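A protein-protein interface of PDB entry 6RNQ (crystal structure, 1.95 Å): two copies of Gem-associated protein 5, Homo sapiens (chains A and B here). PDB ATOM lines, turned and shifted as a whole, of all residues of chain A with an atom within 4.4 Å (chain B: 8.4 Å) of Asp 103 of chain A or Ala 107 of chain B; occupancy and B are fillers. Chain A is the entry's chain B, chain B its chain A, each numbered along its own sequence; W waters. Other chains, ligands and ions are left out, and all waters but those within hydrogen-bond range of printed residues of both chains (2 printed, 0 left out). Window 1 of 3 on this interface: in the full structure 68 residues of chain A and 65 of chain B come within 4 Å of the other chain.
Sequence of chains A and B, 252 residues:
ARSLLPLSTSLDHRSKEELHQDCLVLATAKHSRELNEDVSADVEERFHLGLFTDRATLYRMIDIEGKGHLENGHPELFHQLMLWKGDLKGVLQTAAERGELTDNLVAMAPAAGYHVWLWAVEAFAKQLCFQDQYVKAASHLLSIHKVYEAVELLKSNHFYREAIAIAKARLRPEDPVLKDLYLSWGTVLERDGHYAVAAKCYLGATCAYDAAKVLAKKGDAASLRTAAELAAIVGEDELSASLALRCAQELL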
ATOM      1  N   THR A 102      -7.212 -21.140 -14.379  1.00  0.00           N
ATOM      2  CA  THR A 102      -6.911 -19.738 -14.140  1.00  0.00           C
ATOM      3  C   THR A 102      -6.119 -19.199 -15.321  1.00  0.00           C
ATOM      4  O   THR A 102      -5.581 -19.960 -16.127  1.00  0.00           O
ATOM      5  CB  THR A 102      -6.102 -19.539 -12.848  1.00  0.00           C
ATOM      6  OG1 THR A 102      -4.814 -20.152 -12.994  1.00  0.00           O
ATOM      7  CG2 THR A 102      -6.822 -20.156 -11.655  1.00  0.00           C
ATOM      8  N   ASP A 103      -6.003 -17.906 -15.401  1.00  0.00           N
ATOM      9  CA  ASP A 103      -5.152 -17.253 -16.395  1.00  0.00           C
ATOM     10  C   ASP A 103      -3.731 -17.778 -16.247  1.00  0.00           C
ATOM     11  O   ASP A 103      -3.124 -18.059 -17.226  1.00  0.00           O
ATOM     12  CB  ASP A 103      -5.109 -15.778 -16.120  1.00  0.00           C
ATOM     13  CG  ASP A 103      -6.320 -15.081 -16.653  1.00  0.00           C
ATOM     14  OD1 ASP A 103      -6.537 -15.085 -17.852  1.00  0.00           O
ATOM     15  OD2 ASP A 103      -7.112 -14.581 -15.885  1.00  0.00           O
ATOM     16  N   ASN A 104      -3.270 -17.929 -15.020  1.00  0.00           N
ATOM     17  CA  ASN A 104      -1.901 -18.413 -14.758  1.00  0.00           C
ATOM     18  C   ASN A 104      -1.728 -19.780 -15.389  1.00  0.00           C
ATOM     19  O   ASN A 104      -0.801 -19.929 -16.087  1.00  0.00           O
ATOM     20  CB  ASN A 104      -1.594 -18.493 -13.269  1.00  0.00           C
ATOM     21  CG  ASN A 104      -0.227 -19.069 -12.992  1.00  0.00           C
ATOM     22  OD1 ASN A 104       0.752 -18.425 -13.246  1.00  0.00           O
ATOM     23  ND2 ASN A 104      -0.172 -20.264 -12.470  1.00  0.00           N
ATOM     24  N   LEU A 105      -2.643 -20.704 -15.211  1.00  0.00           N
ATOM     25  CA  LEU A 105      -2.508 -22.047 -15.797  1.00  0.00           C
ATOM     26  C   LEU A 105      -2.640 -22.002 -17.318  1.00  0.00           C
ATOM     27  O   LEU A 105      -1.952 -22.722 -17.976  1.00  0.00           O
ATOM     28  CB  LEU A 105      -3.577 -22.961 -15.220  1.00  0.00           C
ATOM     29  CG  LEU A 105      -3.328 -23.521 -13.830  1.00  0.00           C
ATOM     30  CD1 LEU A 105      -4.345 -24.578 -13.503  1.00  0.00           C
ATOM     31  CD2 LEU A 105      -1.936 -24.100 -13.728  1.00  0.00           C
ATOM     32  N   VAL A 106      -3.526 -21.186 -17.863  1.00  0.00           N
ATOM     33  CA  VAL A 106      -3.707 -21.087 -19.331  1.00  0.00           C
ATOM     34  C   VAL A 106      -2.436 -20.499 -19.946  1.00  0.00           C
ATOM     35  O   VAL A 106      -2.051 -20.942 -20.950  1.00  0.00           O
ATOM     36  CB  VAL A 106      -4.990 -20.337 -19.720  1.00  0.00           C
ATOM     37  CG1 VAL A 106      -5.079 -20.187 -21.213  1.00  0.00           C
ATOM     38  CG2 VAL A 106      -6.212 -21.044 -19.199  1.00  0.00           C
ATOM     39  N   ALA A 107      -1.774 -19.610 -19.248  1.00  0.00           N
ATOM     40  CA  ALA A 107      -0.531 -18.943 -19.663  1.00  0.00           C
ATOM     41  C   ALA A 107       0.609 -19.955 -19.769  1.00  0.00           C
ATOM     42  O   ALA A 107       1.558 -19.655 -20.370  1.00  0.00           O
ATOM     43  CB  ALA A 107      -0.220 -17.843 -18.715  1.00  0.00           C
ATOM     44  N   TRP A 117      -3.057 -25.632 -25.651  1.00  0.00           N
ATOM     45  CA  TRP A 117      -3.498 -24.278 -25.266  1.00  0.00           C
ATOM     46  C   TRP A 117      -4.919 -24.043 -25.765  1.00  0.00           C
ATOM     47  O   TRP A 117      -5.677 -23.516 -25.054  1.00  0.00           O
ATOM     48  CB  TRP A 117      -2.550 -23.252 -25.824  1.00  0.00           C
ATOM     49  CG  TRP A 117      -3.001 -21.847 -25.671  1.00  0.00           C
ATOM     50  CD1 TRP A 117      -3.043 -21.126 -24.538  1.00  0.00           C
ATOM     51  CD2 TRP A 117      -3.463 -20.987 -26.708  1.00  0.00           C
ATOM     52  NE1 TRP A 117      -3.491 -19.879 -24.800  1.00  0.00           N
ATOM     53  CE2 TRP A 117      -3.736 -19.757 -26.124  1.00  0.00           C
ATOM     54  CE3 TRP A 117      -3.646 -21.123 -28.073  1.00  0.00           C
ATOM     55  CZ2 TRP A 117      -4.221 -18.681 -26.844  1.00  0.00           C
ATOM     56  CZ3 TRP A 117      -4.109 -20.057 -28.788  1.00  0.00           C
ATOM     57  CH2 TRP A 117      -4.400 -18.853 -28.182  1.00  0.00           C
ATOM     58  N   PHE A 124     -11.373 -23.050 -20.234  1.00  0.00           N
ATOM     59  CA  PHE A 124     -11.441 -21.889 -19.350  1.00  0.00           C
ATOM     60  C   PHE A 124     -12.678 -21.053 -19.654  1.00  0.00           C
ATOM     61  O   PHE A 124     -13.308 -20.509 -18.739  1.00  0.00           O
ATOM     62  CB  PHE A 124     -10.170 -21.053 -19.501  1.00  0.00           C
ATOM     63  CG  PHE A 124      -9.985 -19.996 -18.434  1.00  0.00           C
ATOM     64  CD1 PHE A 124     -10.524 -20.149 -17.165  1.00  0.00           C
ATOM     65  CD2 PHE A 124      -9.254 -18.850 -18.709  1.00  0.00           C
ATOM     66  CE1 PHE A 124     -10.340 -19.177 -16.194  1.00  0.00           C
ATOM     67  CE2 PHE A 124      -9.069 -17.875 -17.745  1.00  0.00           C
ATOM     68  CZ  PHE A 124      -9.611 -18.038 -16.486  1.00  0.00           C
ATOM     69  N   LYS A 136     -15.501 -11.898 -20.267  1.00  0.00           N
ATOM     70  CA  LYS A 136     -14.139 -12.422 -20.215  1.00  0.00           C
ATOM     71  C   LYS A 136     -14.038 -13.714 -21.014  1.00  0.00           C
ATOM     72  O   LYS A 136     -13.087 -13.909 -21.783  1.00  0.00           O
ATOM     73  CB  LYS A 136     -13.709 -12.645 -18.766  1.00  0.00           C
ATOM     74  CG  LYS A 136     -12.267 -13.129 -18.611  1.00  0.00           C
ATOM     75  CD  LYS A 136     -11.903 -13.313 -17.145  1.00  0.00           C
ATOM     76  CE  LYS A 136     -10.686 -14.221 -16.975  1.00  0.00           C
ATOM     77  NZ  LYS A 136      -9.455 -13.607 -17.525  1.00  0.00           N
ATOM     78  N   HIS A 140     -11.635 -14.712 -24.341  1.00  0.00           N
ATOM     79  CA  HIS A 140     -10.760 -15.871 -24.485  1.00  0.00           C
ATOM     80  C   HIS A 140     -11.076 -16.636 -25.764  1.00  0.00           C
ATOM     81  O   HIS A 140     -10.164 -17.088 -26.465  1.00  0.00           O
ATOM     82  CB  HIS A 140     -10.874 -16.770 -23.254  1.00  0.00           C
ATOM     83  CG  HIS A 140     -10.154 -16.234 -22.056  1.00  0.00           C
ATOM     84  ND1 HIS A 140      -8.778 -16.186 -21.975  1.00  0.00           N
ATOM     85  CD2 HIS A 140     -10.615 -15.719 -20.892  1.00  0.00           C
ATOM     86  CE1 HIS A 140      -8.425 -15.660 -20.816  1.00  0.00           C
ATOM     87  NE2 HIS A 140      -9.520 -15.373 -20.138  1.00  0.00           N
ATOM     88  N   GLU B  76      -6.842  -4.361 -16.952  1.00  0.00           N
ATOM     89  CA  GLU B  76      -7.310  -5.624 -17.524  1.00  0.00           C
ATOM     90  C   GLU B  76      -8.527  -5.411 -18.431  1.00  0.00           C
ATOM     91  O   GLU B  76      -8.752  -6.180 -19.376  1.00  0.00           O
ATOM     92  CB  GLU B  76      -7.658  -6.616 -16.402  1.00  0.00           C
ATOM     93  CG  GLU B  76      -8.873  -6.231 -15.551  1.00  0.00           C
ATOM     94  CD  GLU B  76      -8.589  -5.102 -14.576  1.00  0.00           C
ATOM     95  OE1 GLU B  76      -7.482  -4.508 -14.647  1.00  0.00           O
ATOM     96  OE2 GLU B  76      -9.482  -4.807 -13.743  1.00  0.00           O
ATOM     97  N   LEU B  88      -3.912  -6.397 -29.706  1.00  0.00           N
ATOM     98  CA  LEU B  88      -3.341  -6.944 -28.480  1.00  0.00           C
ATOM     99  C   LEU B  88      -1.847  -7.175 -28.628  1.00  0.00           C
ATOM    100  O   LEU B  88      -1.068  -6.886 -27.713  1.00  0.00           O
ATOM    101  CB  LEU B  88      -4.038  -8.246 -28.130  1.00  0.00           C
ATOM    102  CG  LEU B  88      -3.538  -9.056 -26.924  1.00  0.00           C
ATOM    103  CD1 LEU B  88      -4.116  -8.522 -25.634  1.00  0.00           C
ATOM    104  CD2 LEU B  88      -3.919 -10.509 -27.164  1.00  0.00           C
ATOM    105  N   LEU B  92       0.783  -5.965 -26.033  1.00  0.00           N
ATOM    106  CA  LEU B  92       1.724  -6.791 -25.289  1.00  0.00           C
ATOM    107  C   LEU B  92       3.113  -6.162 -25.270  1.00  0.00           C
ATOM    108  O   LEU B  92       3.779  -6.133 -24.229  1.00  0.00           O
ATOM    109  CB  LEU B  92       1.769  -8.187 -25.894  1.00  0.00           C
ATOM    110  CG  LEU B  92       0.643  -9.107 -25.432  1.00  0.00           C
ATOM    111  CD1 LEU B  92       0.557 -10.320 -26.336  1.00  0.00           C
ATOM    112  CD2 LEU B  92       0.883  -9.525 -23.965  1.00  0.00           C
ATOM    113  N   THR B 102       0.574  -9.260 -17.402  1.00  0.00           N
ATOM    114  CA  THR B 102      -0.295  -9.960 -16.471  1.00  0.00           C
ATOM    115  C   THR B 102      -0.436 -11.406 -16.918  1.00  0.00           C
ATOM    116  O   THR B 102      -0.169 -11.738 -18.074  1.00  0.00           O
ATOM    117  CB  THR B 102      -1.677  -9.307 -16.379  1.00  0.00           C
ATOM    118  OG1 THR B 102      -2.362  -9.465 -17.631  1.00  0.00           O
ATOM    119  CG2 THR B 102      -1.549  -7.817 -16.063  1.00  0.00           C
ATOM    120  N   ASP B 103      -0.862 -12.270 -15.982  1.00  0.00           N
ATOM    121  CA  ASP B 103      -1.190 -13.649 -16.336  1.00  0.00           C
ATOM    122  C   ASP B 103      -2.196 -13.695 -17.484  1.00  0.00           C
ATOM    123  O   ASP B 103      -2.067 -14.510 -18.402  1.00  0.00           O
ATOM    124  CB  ASP B 103      -1.767 -14.390 -15.133  1.00  0.00           C
ATOM    125  CG  ASP B 103      -0.709 -14.744 -14.086  1.00  0.00           C
ATOM    126  OD1 ASP B 103      -0.929 -14.455 -12.888  1.00  0.00           O
ATOM    127  OD2 ASP B 103       0.338 -15.322 -14.458  1.00  0.00           O
ATOM    128  N   ASN B 104      -3.231 -12.851 -17.420  1.00  0.00           N
ATOM    129  CA  ASN B 104      -4.247 -12.815 -18.475  1.00  0.00           C
ATOM    130  C   ASN B 104      -3.639 -12.482 -19.837  1.00  0.00           C
ATOM    131  O   ASN B 104      -3.975 -13.120 -20.845  1.00  0.00           O
ATOM    132  CB  ASN B 104      -5.337 -11.810 -18.083  1.00  0.00           C
ATOM    133  CG  ASN B 104      -6.355 -11.554 -19.197  1.00  0.00           C
ATOM    134  OD1 ASN B 104      -6.364 -10.487 -19.780  1.00  0.00           O
ATOM    135  ND2 ASN B 104      -7.212 -12.531 -19.480  1.00  0.00           N
ATOM    136  N   LEU B 105      -2.733 -11.508 -19.896  1.00  0.00           N
ATOM    137  CA  LEU B 105      -2.135 -11.159 -21.183  1.00  0.00           C
ATOM    138  C   LEU B 105      -1.304 -12.309 -21.742  1.00  0.00           C
ATOM    139  O   LEU B 105      -1.314 -12.565 -22.951  1.00  0.00           O
ATOM    140  CB  LEU B 105      -1.271  -9.908 -21.054  1.00  0.00           C
ATOM    141  CG  LEU B 105      -2.004  -8.564 -21.120  1.00  0.00           C
ATOM    142  CD1 LEU B 105      -1.010  -7.411 -20.883  1.00  0.00           C
ATOM    143  CD2 LEU B 105      -2.709  -8.366 -22.438  1.00  0.00           C
ATOM    144  N   VAL B 106      -0.581 -13.025 -20.882  1.00  0.00           N
ATOM    145  CA  VAL B 106       0.208 -14.149 -21.372  1.00  0.00           C
ATOM    146  C   VAL B 106      -0.706 -15.281 -21.820  1.00  0.00           C
ATOM    147  O   VAL B 106      -0.416 -15.983 -22.796  1.00  0.00           O
ATOM    148  CB  VAL B 106       1.205 -14.617 -20.298  1.00  0.00           C
ATOM    149  CG1 VAL B 106       2.026 -15.800 -20.805  1.00  0.00           C
ATOM    150  CG2 VAL B 106       2.108 -13.475 -19.896  1.00  0.00           C
ATOM    151  N   ALA B 107      -1.826 -15.477 -21.118  1.00  0.00           N
ATOM    152  CA  ALA B 107      -2.763 -16.532 -21.497  1.00  0.00           C
ATOM    153  C   ALA B 107      -3.357 -16.302 -22.882  1.00  0.00           C
ATOM    154  O   ALA B 107      -3.757 -17.266 -23.558  1.00  0.00           O
ATOM    155  CB  ALA B 107      -3.893 -16.636 -20.459  1.00  0.00           C
ATOM    156  N   MET B 108      -3.454 -15.040 -23.314  1.00  0.00           N
ATOM    157  CA  MET B 108      -3.969 -14.724 -24.637  1.00  0.00           C
ATOM    158  C   MET B 108      -2.880 -14.540 -25.681  1.00  0.00           C
ATOM    159  O   MET B 108      -3.198 -14.494 -26.876  1.00  0.00           O
ATOM    160  CB  MET B 108      -4.828 -13.452 -24.591  1.00  0.00           C
ATOM    161  CG  MET B 108      -5.978 -13.518 -23.603  1.00  0.00           C
ATOM    162  SD  MET B 108      -7.055 -12.102 -23.734  1.00  0.00           S
ATOM    163  CE  MET B 108      -5.985 -10.746 -23.291  1.00  0.00           C
ATOM    164  N   ALA B 109      -1.621 -14.429 -25.262  1.00  0.00           N
ATOM    165  CA  ALA B 109      -0.541 -14.101 -26.182  1.00  0.00           C
ATOM    166  C   ALA B 109      -0.430 -15.023 -27.388  1.00  0.00           C
ATOM    167  O   ALA B 109      -0.136 -14.521 -28.479  1.00  0.00           O
ATOM    168  CB  ALA B 109       0.799 -14.083 -25.436  1.00  0.00           C
ATOM    169  N   PRO B 110      -0.626 -16.350 -27.263  1.00  0.00           N
ATOM    170  CA  PRO B 110      -0.494 -17.210 -28.462  1.00  0.00           C
ATOM    171  C   PRO B 110      -1.459 -16.842 -29.591  1.00  0.00           C
ATOM    172  O   PRO B 110      -1.297 -17.332 -30.720  1.00  0.00           O
ATOM    173  CB  PRO B 110      -0.779 -18.622 -27.916  1.00  0.00           C
ATOM    174  CG  PRO B 110      -0.560 -18.525 -26.453  1.00  0.00           C
ATOM    175  CD  PRO B 110      -0.970 -17.128 -26.057  1.00  0.00           C
ATOM    176  N   ALA B 111      -2.474 -16.021 -29.321  1.00  0.00           N
ATOM    177  CA  ALA B 111      -3.326 -15.537 -30.402  1.00  0.00           C
ATOM    178  C   ALA B 111      -2.506 -14.798 -31.454  1.00  0.00           C
ATOM    179  O   ALA B 111      -2.862 -14.799 -32.630  1.00  0.00           O
ATOM    180  CB  ALA B 111      -4.410 -14.624 -29.844  1.00  0.00           C
ATOM    181  N   TRP B 117       4.013 -15.681 -27.675  1.00  0.00           N
ATOM    182  CA  TRP B 117       3.835 -16.196 -26.318  1.00  0.00           C
ATOM    183  C   TRP B 117       5.188 -16.455 -25.664  1.00  0.00           C
ATOM    184  O   TRP B 117       5.428 -16.048 -24.523  1.00  0.00           O
ATOM    185  CB  TRP B 117       2.999 -17.476 -26.346  1.00  0.00           C
ATOM    186  CG  TRP B 117       3.017 -18.230 -25.049  1.00  0.00           C
ATOM    187  CD1 TRP B 117       2.299 -17.947 -23.926  1.00  0.00           C
ATOM    188  CD2 TRP B 117       3.808 -19.385 -24.740  1.00  0.00           C
ATOM    189  NE1 TRP B 117       2.605 -18.857 -22.926  1.00  0.00           N
ATOM    190  CE2 TRP B 117       3.520 -19.751 -23.413  1.00  0.00           C
ATOM    191  CE3 TRP B 117       4.732 -20.146 -25.459  1.00  0.00           C
ATOM    192  CZ2 TRP B 117       4.122 -20.844 -22.792  1.00  0.00           C
ATOM    193  CZ3 TRP B 117       5.330 -21.233 -24.833  1.00  0.00           C
ATOM    194  CH2 TRP B 117       5.005 -21.579 -23.522  1.00  0.00           C
ATOM    195  N   ALA B 120       6.501 -13.283 -24.685  1.00  0.00           N
ATOM    196  CA  ALA B 120       5.744 -12.724 -23.567  1.00  0.00           C
ATOM    197  C   ALA B 120       6.095 -13.413 -22.247  1.00  0.00           C
ATOM    198  O   ALA B 120       6.143 -12.765 -21.198  1.00  0.00           O
ATOM    199  CB  ALA B 120       4.242 -12.833 -23.839  1.00  0.00           C
ATOM    200  N   VAL B 121       6.319 -14.725 -22.270  1.00  0.00           N
ATOM    201  CA  VAL B 121       6.681 -15.429 -21.038  1.00  0.00           C
ATOM    202  C   VAL B 121       8.037 -14.947 -20.520  1.00  0.00           C
ATOM    203  O   VAL B 121       8.212 -14.696 -19.322  1.00  0.00           O
ATOM    204  CB  VAL B 121       6.684 -16.945 -21.281  1.00  0.00           C
ATOM    205  CG1 VAL B 121       7.313 -17.699 -20.049  1.00  0.00           C
ATOM    206  CG2 VAL B 121       5.292 -17.441 -21.543  1.00  0.00           C
ATOM    207  N   PHE B 124       7.575 -11.595 -19.098  1.00  0.00           N
ATOM    208  CA  PHE B 124       6.833 -11.698 -17.843  1.00  0.00           C
ATOM    209  C   PHE B 124       7.719 -12.198 -16.697  1.00  0.00           C
ATOM    210  O   PHE B 124       7.626 -11.699 -15.569  1.00  0.00           O
ATOM    211  CB  PHE B 124       5.638 -12.625 -18.038  1.00  0.00           C
ATOM    212  CG  PHE B 124       4.642 -12.583 -16.916  1.00  0.00           C
ATOM    213  CD1 PHE B 124       4.354 -11.390 -16.277  1.00  0.00           C
ATOM    214  CD2 PHE B 124       3.947 -13.730 -16.538  1.00  0.00           C
ATOM    215  CE1 PHE B 124       3.416 -11.341 -15.266  1.00  0.00           C
ATOM    216  CE2 PHE B 124       2.995 -13.683 -15.548  1.00  0.00           C
ATOM    217  CZ  PHE B 124       2.736 -12.497 -14.898  1.00  0.00           C
ATOM    218  N   LYS B 136       7.317 -17.582  -8.633  1.00  0.00           N
ATOM    219  CA  LYS B 136       6.401 -17.526  -9.763  1.00  0.00           C
ATOM    220  C   LYS B 136       7.161 -17.335 -11.079  1.00  0.00           C
ATOM    221  O   LYS B 136       6.857 -17.990 -12.086  1.00  0.00           O
ATOM    222  CB  LYS B 136       5.388 -16.408  -9.545  1.00  0.00           C
ATOM    223  CG  LYS B 136       4.393 -16.240 -10.704  1.00  0.00           C
ATOM    224  CD  LYS B 136       3.353 -15.169 -10.372  1.00  0.00           C
ATOM    225  CE  LYS B 136       2.504 -14.811 -11.593  1.00  0.00           C
ATOM    226  NZ  LYS B 136       1.877 -16.013 -12.205  1.00  0.00           N
ATOM    227  N   HIS B 140       7.208 -19.798 -14.655  1.00  0.00           N
ATOM    228  CA  HIS B 140       7.006 -19.437 -16.062  1.00  0.00           C
ATOM    229  C   HIS B 140       8.210 -19.804 -16.909  1.00  0.00           C
ATOM    230  O   HIS B 140       8.043 -20.240 -18.046  1.00  0.00           O
ATOM    231  CB  HIS B 140       6.670 -17.955 -16.176  1.00  0.00           C
ATOM    232  CG  HIS B 140       5.313 -17.621 -15.633  1.00  0.00           C
ATOM    233  ND1 HIS B 140       4.149 -17.926 -16.305  1.00  0.00           N
ATOM    234  CD2 HIS B 140       4.929 -17.042 -14.470  1.00  0.00           C
ATOM    235  CE1 HIS B 140       3.108 -17.555 -15.581  1.00  0.00           C
ATOM    236  NE2 HIS B 140       3.553 -16.997 -14.470  1.00  0.00           N
HETATM  237  O   HOH W   1      -6.573 -16.836 -23.835  1.00  0.00           O
HETATM  238  O   HOH W   2       3.970 -19.097 -19.024  1.00  0.00           O
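ND2 of Asn 104 of chain B sits close to NZ of Lys 136 of chain A.
A ring nitrogen (NE2) of His 140 of chain B is in hydrogen-bond range of the side-chain amide oxygen (OD1) of Asn 104 of chain A, at 3.4 Å.
OD1 of Asn 104 of chain A lies close to OD2 of Asp 103 of chain B (3.4 Å).
The backbone carbonyl oxygen (O) of Ala 107 of chain A is in hydrogen-bond range of the indole nitrogen (NE1) of Trp 117 of chain B.
The side-chain amino group (NZ) of Lys 136 of chain B is in hydrogen-bond range of the side-chain amide oxygen (OD1) of Asn 104 of chain A, at 2.9 Å.
ND2 of Asn 104 of chain B is in hydrogen-bond range of OD1 of Asp 103 of chain A (3.1 Å).
The backbone carbonyl oxygen (O) of Ala 107 of chain B lies within hydrogen-bond range of the indole nitrogen (NE1) of Trp 117 of chain A (2.9 Å).
The side-chain amino group of Lys 136 of chain B lies within hydrogen-bond range of a ring nitrogen (NE2) of His 140 of chain B, at 3.0 Å.
The backbone NH (N) of Asn 104 of chain A lies close to the side-chain hydroxyl (OG1) of Thr 102 of chain A (3.4 Å).
The side-chain amino group (NZ) of Lys 136 of chain A lies within hydrogen-bond range of a ring nitrogen (NE2) of His 140 of chain A, at 3.2 Å.
The side-chain amino group (NZ) of Lys 136 of chain B is in salt-bridge range of the side-chain carboxylate (OD2) of Asp 103 of chain B, at 2.8 Å.
The side-chain carboxylate of Asp 103 of chain A lies within salt-bridge range of the side-chain amino group of Lys 136 of chain A (3.0 Å).
Among the printed residues, pairs that only touch across the chains: Asp 103 of chain A with Asp 103 of chain B (3.8 Å), Asp 103 of chain A with Ala 107 of chain B (3.6 Å), Val 106 of chain A with Ala 107 of chain B (3.8 Å), Ala 107 of chain A with Asp 103 of chain B (3.8 Å), Ala 107 of chain A with Val 106 of chain B (3.7 Å), Ala 107 of chain A with Ala 107 of chain B (3.7 Å), Trp 117 of chain A with Pro 110 of chain B (3.4 Å), Trp 117 of chain A with Ala 111 of chain B (3.6 Å) and His 140 of chain A with Asn 104 of chain B (3.6 Å).
Asp 103 of chain A touches three residues of chain B.
Of chain A, only Asp 103, Val 106, Ala 107 and Trp 117 come within 4 Å of Ala 107 of chain B.
Of the printed residues of chain B, Lys 136 of chain A touches Asn 104 (3.2 Å).
Of the printed residues of chain A, Asn 104 of chain B touches Asp 103, Lys 136 and His 140.
Printed residues of chain B within 4 Å of Trp 117 of chain A: Ala 107, Pro 110 and Ala 111.
Printed residues of chain A within 4 Å of His 140 of chain B: Asn 104.
Ala 109 of chain B touches none of the printed residues of chain A.
Glu 76 of chain B touches none of the printed residues of chain A.
The nearest residue of chain B that does not touch Asp 103 of chain A is Leu 105 of chain B (5.6 Å).
Of the 10 printed residues of chain A, 7 touch a printed residue of chain B.
Asp 103 of chain A touches its own counterpart, Asp 103 of chain B.
Asp 103 of chain A touches Ala 107 of chain B, and with the chains exchanged Ala 107 of chain A touches Asp 103 of chain B.
Asn 104 of chain A touches Lys 136 of chain B, and with the chains exchanged Lys 136 of chain A touches Asn 104 of chain B.
Ala 107 of chain A touches its own counterpart, Ala 107 of chain B.
Of the 16 pairs that touch across the chains among the printed residues, 14 have their exchanged pair printed and touching as well.
Water W2 bridges O of Ala 107 of chain A and ND1 of His 140 of chain B.
Water W1 lies within hydrogen-bond range of O of Ala 107 of chain B (2.9 Å) and ND1 of His 140 of chain A (3.0 Å).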
